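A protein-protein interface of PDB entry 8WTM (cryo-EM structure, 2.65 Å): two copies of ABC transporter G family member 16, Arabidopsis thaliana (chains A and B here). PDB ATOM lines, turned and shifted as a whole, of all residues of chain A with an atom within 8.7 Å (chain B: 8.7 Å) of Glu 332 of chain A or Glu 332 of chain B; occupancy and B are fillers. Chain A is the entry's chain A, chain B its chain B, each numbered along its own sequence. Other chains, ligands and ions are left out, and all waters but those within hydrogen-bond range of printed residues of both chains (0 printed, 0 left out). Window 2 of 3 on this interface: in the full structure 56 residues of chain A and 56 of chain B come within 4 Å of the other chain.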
ATOM      1  N   HIS A 293      17.537 -33.255  26.939  1.00  0.00           N
ATOM      2  CA  HIS A 293      17.743 -33.309  25.497  1.00  0.00           C
ATOM      3  C   HIS A 293      18.611 -34.486  25.077  1.00  0.00           C
ATOM      4  O   HIS A 293      18.565 -34.888  23.911  1.00  0.00           O
ATOM      5  CB  HIS A 293      18.368 -32.004  25.005  1.00  0.00           C
ATOM      6  CG  HIS A 293      17.368 -30.990  24.543  1.00  0.00           C
ATOM      7  ND1 HIS A 293      17.607 -29.634  24.589  1.00  0.00           N
ATOM      8  CD2 HIS A 293      16.141 -31.138  23.993  1.00  0.00           C
ATOM      9  CE1 HIS A 293      16.559 -28.988  24.109  1.00  0.00           C
ATOM     10  NE2 HIS A 293      15.656 -29.878  23.740  1.00  0.00           N
ATOM     11  N   PRO A 320       6.787 -31.363  17.457  1.00  0.00           N
ATOM     12  CA  PRO A 320       6.441 -30.064  16.855  1.00  0.00           C
ATOM     13  C   PRO A 320       5.293 -30.144  15.868  1.00  0.00           C
ATOM     14  O   PRO A 320       4.497 -29.202  15.780  1.00  0.00           O
ATOM     15  CB  PRO A 320       7.746 -29.634  16.173  1.00  0.00           C
ATOM     16  CG  PRO A 320       8.789 -30.288  16.942  1.00  0.00           C
ATOM     17  CD  PRO A 320       8.232 -31.627  17.262  1.00  0.00           C
ATOM     18  N   PRO A 329       2.418 -23.953  18.619  1.00  0.00           N
ATOM     19  CA  PRO A 329       3.655 -24.690  18.338  1.00  0.00           C
ATOM     20  C   PRO A 329       4.690 -24.500  19.439  1.00  0.00           C
ATOM     21  O   PRO A 329       4.508 -23.748  20.396  1.00  0.00           O
ATOM     22  CB  PRO A 329       4.138 -24.091  17.012  1.00  0.00           C
ATOM     23  CG  PRO A 329       2.963 -23.325  16.469  1.00  0.00           C
ATOM     24  CD  PRO A 329       2.212 -22.854  17.663  1.00  0.00           C
ATOM     25  N   ILE A 330       5.798 -25.216  19.281  1.00  0.00           N
ATOM     26  CA  ILE A 330       6.884 -25.230  20.257  1.00  0.00           C
ATOM     27  C   ILE A 330       7.953 -24.251  19.786  1.00  0.00           C
ATOM     28  O   ILE A 330       8.371 -24.310  18.622  1.00  0.00           O
ATOM     29  CB  ILE A 330       7.460 -26.647  20.448  1.00  0.00           C
ATOM     30  CG1 ILE A 330       6.431 -27.587  21.080  1.00  0.00           C
ATOM     31  CG2 ILE A 330       8.708 -26.628  21.320  1.00  0.00           C
ATOM     32  CD1 ILE A 330       5.633 -28.410  20.112  1.00  0.00           C
ATOM     33  N   PRO A 331       8.412 -23.338  20.639  1.00  0.00           N
ATOM     34  CA  PRO A 331       9.426 -22.370  20.210  1.00  0.00           C
ATOM     35  C   PRO A 331      10.800 -23.003  20.053  1.00  0.00           C
ATOM     36  O   PRO A 331      11.076 -24.103  20.534  1.00  0.00           O
ATOM     37  CB  PRO A 331       9.429 -21.330  21.339  1.00  0.00           C
ATOM     38  CG  PRO A 331       8.182 -21.593  22.129  1.00  0.00           C
ATOM     39  CD  PRO A 331       7.929 -23.055  21.998  1.00  0.00           C
ATOM     40  N   GLU A 332      11.667 -22.276  19.356  1.00  0.00           N
ATOM     41  CA  GLU A 332      13.060 -22.660  19.211  1.00  0.00           C
ATOM     42  C   GLU A 332      13.781 -22.431  20.537  1.00  0.00           C
ATOM     43  O   GLU A 332      13.395 -21.559  21.324  1.00  0.00           O
ATOM     44  CB  GLU A 332      13.708 -21.845  18.084  1.00  0.00           C
ATOM     45  CG  GLU A 332      15.111 -22.264  17.652  1.00  0.00           C
ATOM     46  CD  GLU A 332      15.134 -23.586  16.911  1.00  0.00           C
ATOM     47  OE1 GLU A 332      14.112 -23.934  16.282  1.00  0.00           O
ATOM     48  OE2 GLU A 332      16.174 -24.276  16.952  1.00  0.00           O
ATOM     49  N   ASN A 333      14.813 -23.254  20.785  1.00  0.00           N
ATOM     50  CA  ASN A 333      15.611 -23.255  22.020  1.00  0.00           C
ATOM     51  C   ASN A 333      14.742 -23.504  23.253  1.00  0.00           C
ATOM     52  O   ASN A 333      14.966 -22.938  24.324  1.00  0.00           O
ATOM     53  CB  ASN A 333      16.434 -21.970  22.176  1.00  0.00           C
ATOM     54  CG  ASN A 333      17.556 -21.868  21.159  1.00  0.00           C
ATOM     55  OD1 ASN A 333      18.235 -22.852  20.864  1.00  0.00           O
ATOM     56  ND2 ASN A 333      17.756 -20.672  20.618  1.00  0.00           N
ATOM     57  N   GLU A 334      13.739 -24.361  23.091  1.00  0.00           N
ATOM     58  CA  GLU A 334      12.894 -24.823  24.181  1.00  0.00           C
ATOM     59  C   GLU A 334      12.932 -26.341  24.189  1.00  0.00           C
ATOM     60  O   GLU A 334      12.964 -26.973  23.130  1.00  0.00           O
ATOM     61  CB  GLU A 334      11.449 -24.331  24.032  1.00  0.00           C
ATOM     62  CG  GLU A 334      11.261 -22.835  24.243  1.00  0.00           C
ATOM     63  CD  GLU A 334      11.416 -22.418  25.696  1.00  0.00           C
ATOM     64  OE1 GLU A 334      11.059 -23.218  26.586  1.00  0.00           O
ATOM     65  OE2 GLU A 334      11.892 -21.290  25.946  1.00  0.00           O
ATOM     66  N   ASN A 335      12.960 -26.919  25.386  1.00  0.00           N
ATOM     67  CA  ASN A 335      13.022 -28.367  25.518  1.00  0.00           C
ATOM     68  C   ASN A 335      11.675 -28.976  25.154  1.00  0.00           C
ATOM     69  O   ASN A 335      10.650 -28.637  25.752  1.00  0.00           O
ATOM     70  CB  ASN A 335      13.418 -28.747  26.943  1.00  0.00           C
ATOM     71  CG  ASN A 335      13.620 -30.240  27.119  1.00  0.00           C
ATOM     72  OD1 ASN A 335      13.939 -30.951  26.173  1.00  0.00           O
ATOM     73  ND2 ASN A 335      13.430 -30.720  28.337  1.00  0.00           N
ATOM     74  N   GLN A 336      11.670 -29.848  24.151  1.00  0.00           N
ATOM     75  CA  GLN A 336      10.487 -30.645  23.882  1.00  0.00           C
ATOM     76  C   GLN A 336      10.344 -31.714  24.956  1.00  0.00           C
ATOM     77  O   GLN A 336      11.314 -32.070  25.632  1.00  0.00           O
ATOM     78  CB  GLN A 336      10.561 -31.270  22.492  1.00  0.00           C
ATOM     79  CG  GLN A 336      10.104 -30.334  21.391  1.00  0.00           C
ATOM     80  CD  GLN A 336      10.939 -30.452  20.139  1.00  0.00           C
ATOM     81  OE1 GLN A 336      11.477 -31.514  19.835  1.00  0.00           O
ATOM     82  NE2 GLN A 336      11.059 -29.353  19.404  1.00  0.00           N
ATOM     83  N   HIS B 293      15.270 -23.856  30.260  1.00  0.00           N
ATOM     84  CA  HIS B 293      15.298 -22.858  29.198  1.00  0.00           C
ATOM     85  C   HIS B 293      14.439 -21.645  29.520  1.00  0.00           C
ATOM     86  O   HIS B 293      14.649 -20.580  28.930  1.00  0.00           O
ATOM     87  CB  HIS B 293      14.842 -23.481  27.879  1.00  0.00           C
ATOM     88  CG  HIS B 293      15.964 -24.002  27.036  1.00  0.00           C
ATOM     89  ND1 HIS B 293      15.805 -25.039  26.143  1.00  0.00           N
ATOM     90  CD2 HIS B 293      17.253 -23.605  26.926  1.00  0.00           C
ATOM     91  CE1 HIS B 293      16.953 -25.274  25.536  1.00  0.00           C
ATOM     92  NE2 HIS B 293      17.848 -24.418  25.992  1.00  0.00           N
ATOM     93  N   PRO B 320      27.511 -19.723  23.767  1.00  0.00           N
ATOM     94  CA  PRO B 320      28.028 -20.329  22.528  1.00  0.00           C
ATOM     95  C   PRO B 320      29.314 -19.692  22.038  1.00  0.00           C
ATOM     96  O   PRO B 320      30.169 -20.392  21.485  1.00  0.00           O
ATOM     97  CB  PRO B 320      26.880 -20.127  21.531  1.00  0.00           C
ATOM     98  CG  PRO B 320      25.688 -20.073  22.359  1.00  0.00           C
ATOM     99  CD  PRO B 320      26.103 -19.309  23.562  1.00  0.00           C
ATOM    100  N   PRO B 329      32.079 -26.332  20.478  1.00  0.00           N
ATOM    101  CA  PRO B 329      30.861 -25.517  20.553  1.00  0.00           C
ATOM    102  C   PRO B 329      29.674 -26.318  21.073  1.00  0.00           C
ATOM    103  O   PRO B 329      29.744 -27.522  21.316  1.00  0.00           O
ATOM    104  CB  PRO B 329      30.636 -25.070  19.103  1.00  0.00           C
ATOM    105  CG  PRO B 329      31.928 -25.362  18.392  1.00  0.00           C
ATOM    106  CD  PRO B 329      32.504 -26.546  19.086  1.00  0.00           C
ATOM    107  N   ILE B 330      28.565 -25.608  21.246  1.00  0.00           N
ATOM    108  CA  ILE B 330      27.336 -26.171  21.800  1.00  0.00           C
ATOM    109  C   ILE B 330      26.420 -26.535  20.637  1.00  0.00           C
ATOM    110  O   ILE B 330      26.193 -25.702  19.749  1.00  0.00           O
ATOM    111  CB  ILE B 330      26.652 -25.194  22.775  1.00  0.00           C
ATOM    112  CG1 ILE B 330      27.505 -24.963  24.023  1.00  0.00           C
ATOM    113  CG2 ILE B 330      25.282 -25.703  23.204  1.00  0.00           C
ATOM    114  CD1 ILE B 330      28.398 -23.758  23.979  1.00  0.00           C
ATOM    115  N   PRO B 331      25.885 -27.752  20.593  1.00  0.00           N
ATOM    116  CA  PRO B 331      25.016 -28.139  19.478  1.00  0.00           C
ATOM    117  C   PRO B 331      23.649 -27.476  19.555  1.00  0.00           C
ATOM    118  O   PRO B 331      23.231 -26.945  20.586  1.00  0.00           O
ATOM    119  CB  PRO B 331      24.893 -29.661  19.630  1.00  0.00           C
ATOM    120  CG  PRO B 331      25.977 -30.057  20.587  1.00  0.00           C
ATOM    121  CD  PRO B 331      26.158 -28.886  21.489  1.00  0.00           C
ATOM    122  N   GLU B 332      22.953 -27.513  18.423  1.00  0.00           N
ATOM    123  CA  GLU B 332      21.581 -27.044  18.342  1.00  0.00           C
ATOM    124  C   GLU B 332      20.669 -28.041  19.054  1.00  0.00           C
ATOM    125  O   GLU B 332      20.975 -29.236  19.126  1.00  0.00           O
ATOM    126  CB  GLU B 332      21.175 -26.880  16.872  1.00  0.00           C
ATOM    127  CG  GLU B 332      19.838 -26.196  16.600  1.00  0.00           C
ATOM    128  CD  GLU B 332      19.855 -24.713  16.916  1.00  0.00           C
ATOM    129  OE1 GLU B 332      20.942 -24.101  16.845  1.00  0.00           O
ATOM    130  OE2 GLU B 332      18.781 -24.156  17.229  1.00  0.00           O
ATOM    131  N   ASN B 333      19.562 -27.521  19.609  1.00  0.00           N
ATOM    132  CA  ASN B 333      18.576 -28.282  20.391  1.00  0.00           C
ATOM    133  C   ASN B 333      19.218 -28.954  21.605  1.00  0.00           C
ATOM    134  O   ASN B 333      18.858 -30.068  21.987  1.00  0.00           O
ATOM    135  CB  ASN B 333      17.819 -29.301  19.530  1.00  0.00           C
ATOM    136  CG  ASN B 333      16.885 -28.642  18.532  1.00  0.00           C
ATOM    137  OD1 ASN B 333      16.204 -27.666  18.849  1.00  0.00           O
ATOM    138  ND2 ASN B 333      16.849 -29.176  17.317  1.00  0.00           N
ATOM    139  N   GLU B 334      20.179 -28.264  22.210  1.00  0.00           N
ATOM    140  CA  GLU B 334      20.806 -28.681  23.453  1.00  0.00           C
ATOM    141  C   GLU B 334      20.675 -27.542  24.448  1.00  0.00           C
ATOM    142  O   GLU B 334      20.777 -26.370  24.076  1.00  0.00           O
ATOM    143  CB  GLU B 334      22.283 -29.043  23.255  1.00  0.00           C
ATOM    144  CG  GLU B 334      22.526 -30.319  22.462  1.00  0.00           C
ATOM    145  CD  GLU B 334      22.164 -31.575  23.235  1.00  0.00           C
ATOM    146  OE1 GLU B 334      22.322 -31.578  24.474  1.00  0.00           O
ATOM    147  OE2 GLU B 334      21.723 -32.560  22.604  1.00  0.00           O
ATOM    148  N   ASN B 335      20.418 -27.888  25.705  1.00  0.00           N
ATOM    149  CA  ASN B 335      20.246 -26.881  26.742  1.00  0.00           C
ATOM    150  C   ASN B 335      21.595 -26.266  27.090  1.00  0.00           C
ATOM    151  O   ASN B 335      22.528 -26.976  27.476  1.00  0.00           O
ATOM    152  CB  ASN B 335      19.603 -27.505  27.978  1.00  0.00           C
ATOM    153  CG  ASN B 335      19.284 -26.483  29.053  1.00  0.00           C
ATOM    154  OD1 ASN B 335      19.079 -25.309  28.768  1.00  0.00           O
ATOM    155  ND2 ASN B 335      19.244 -26.931  30.297  1.00  0.00           N
ATOM    156  N   GLN B 336      21.709 -24.953  26.922  1.00  0.00           N
ATOM    157  CA  GLN B 336      22.869 -24.249  27.437  1.00  0.00           C
ATOM    158  C   GLN B 336      22.770 -24.156  28.954  1.00  0.00           C
ATOM    159  O   GLN B 336      21.684 -24.271  29.529  1.00  0.00           O
ATOM    160  CB  GLN B 336      22.983 -22.864  26.810  1.00  0.00           C
ATOM    161  CG  GLN B 336      23.668 -22.874  25.458  1.00  0.00           C
ATOM    162  CD  GLN B 336      23.041 -21.914  24.476  1.00  0.00           C
ATOM    163  OE1 GLN B 336      22.496 -20.882  24.861  1.00  0.00           O
ATOM    164  NE2 GLN B 336      23.111 -22.252  23.195  1.00  0.00           N
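His 293 of chain B touches His 293 of chain A (CE1 to CE1, 3.998 Å).
His 293 of chain A touches Glu 334 of chain B.
Asn 333 of chain B touches Glu 332 of chain A (OD1 to OE2, 3.9 Å).
OD1 of Asn 333 of chain A touches OE2 of Glu 332 of chain B (3.9 Å).
Glu 334 of chain A touches His 293 of chain B (CA to ND1, 3.5 Å).
Printed residues of chain A that touch a printed residue of chain B: His 293, Glu 332, Asn 333, Glu 334 and Asn 335.
Along chain A the printed residues that touch a printed residue of chain B span positions 293 to 335.
Hydrophobic or aromatic side chains of chain B that line the printed part of chain A: His 293.
OD1 of Asn 335 of chain A sits close to NE2 of His 293 of chain A, 3.2 Å away.
The side-chain amide oxygen (OD1) of Asn 335 of chain B sits close to a ring nitrogen (NE2) of His 293 of chain B, 3.2 Å away.
A ring nitrogen (ND1) of His 293 of chain A is in hydrogen-bond range of the backbone carbonyl oxygen (O) of Asn 333 of chain B, 2.9 Å away.
The backbone NH of Asn 335 of chain B is in hydrogen-bond range of a ring nitrogen (ND1) of His 293 of chain A, at 3.5 Å.
OE2 of Glu 332 of chain A sits close to OE2 of Glu 332 of chain B, 2.6 Å away.
The backbone carbonyl oxygen (O) of Asn 333 of chain A is in hydrogen-bond range of a ring nitrogen (ND1) of His 293 of chain B, 2.9 Å away.
A ring nitrogen (ND1) of His 293 of chain B sits at hydrogen-bond distance from the backbone NH of Asn 335 of chain A, 3.5 Å away.
His 293 of chain A touches Asn 333 of chain B, and with the chains exchanged Asn 333 of chain A touches His 293 of chain B.
His 293 of chain A touches Glu 334 of chain B, and with the chains exchanged Glu 334 of chain A touches His 293 of chain B.
His 293 of chain A touches Asn 335 of chain B, and with the chains exchanged Asn 335 of chain A touches His 293 of chain B.
Glu 332 of chain A touches its own counterpart, Glu 332 of chain B.
Positions printed for both chains: 293, 320, 329, 330, 331, 332, 333, 334, 335 and 336.
Of the 10 pairs that touch across the chains among the printed residues, 10 have their exchanged pair printed and touching as well.
Printed residues of chain B within 4 Å of His 293 of chain A: His 293, Asn 333, Glu 334 and Asn 335.
Pro 320 of chain A touches none of the printed residues of chain B.
Pro 329 of chain A touches none of the printed residues of chain B.
No residue of chain B comes within 4 Å of Pro 331 of chain A.
Glu 332 of chain A touches two residues of chain B.
Of chain B, only His 293 and Glu 332 come within 4 Å of Asn 333 of chain A.
Of the printed residues of chain B, Asn 335 of chain A touches His 293.
Glu 332 of chain B touches just these residues of chain A: Glu 332 (2.6 Å) and Asn 333 (3.9 Å).
Printed residues of chain A within 4 Å of Glu 334 of chain B: His 293 (3.5 Å).
The nearest printed residue of chain A that does not touch His 293 of chain B is Glu 332 of chain A (6.4 Å).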
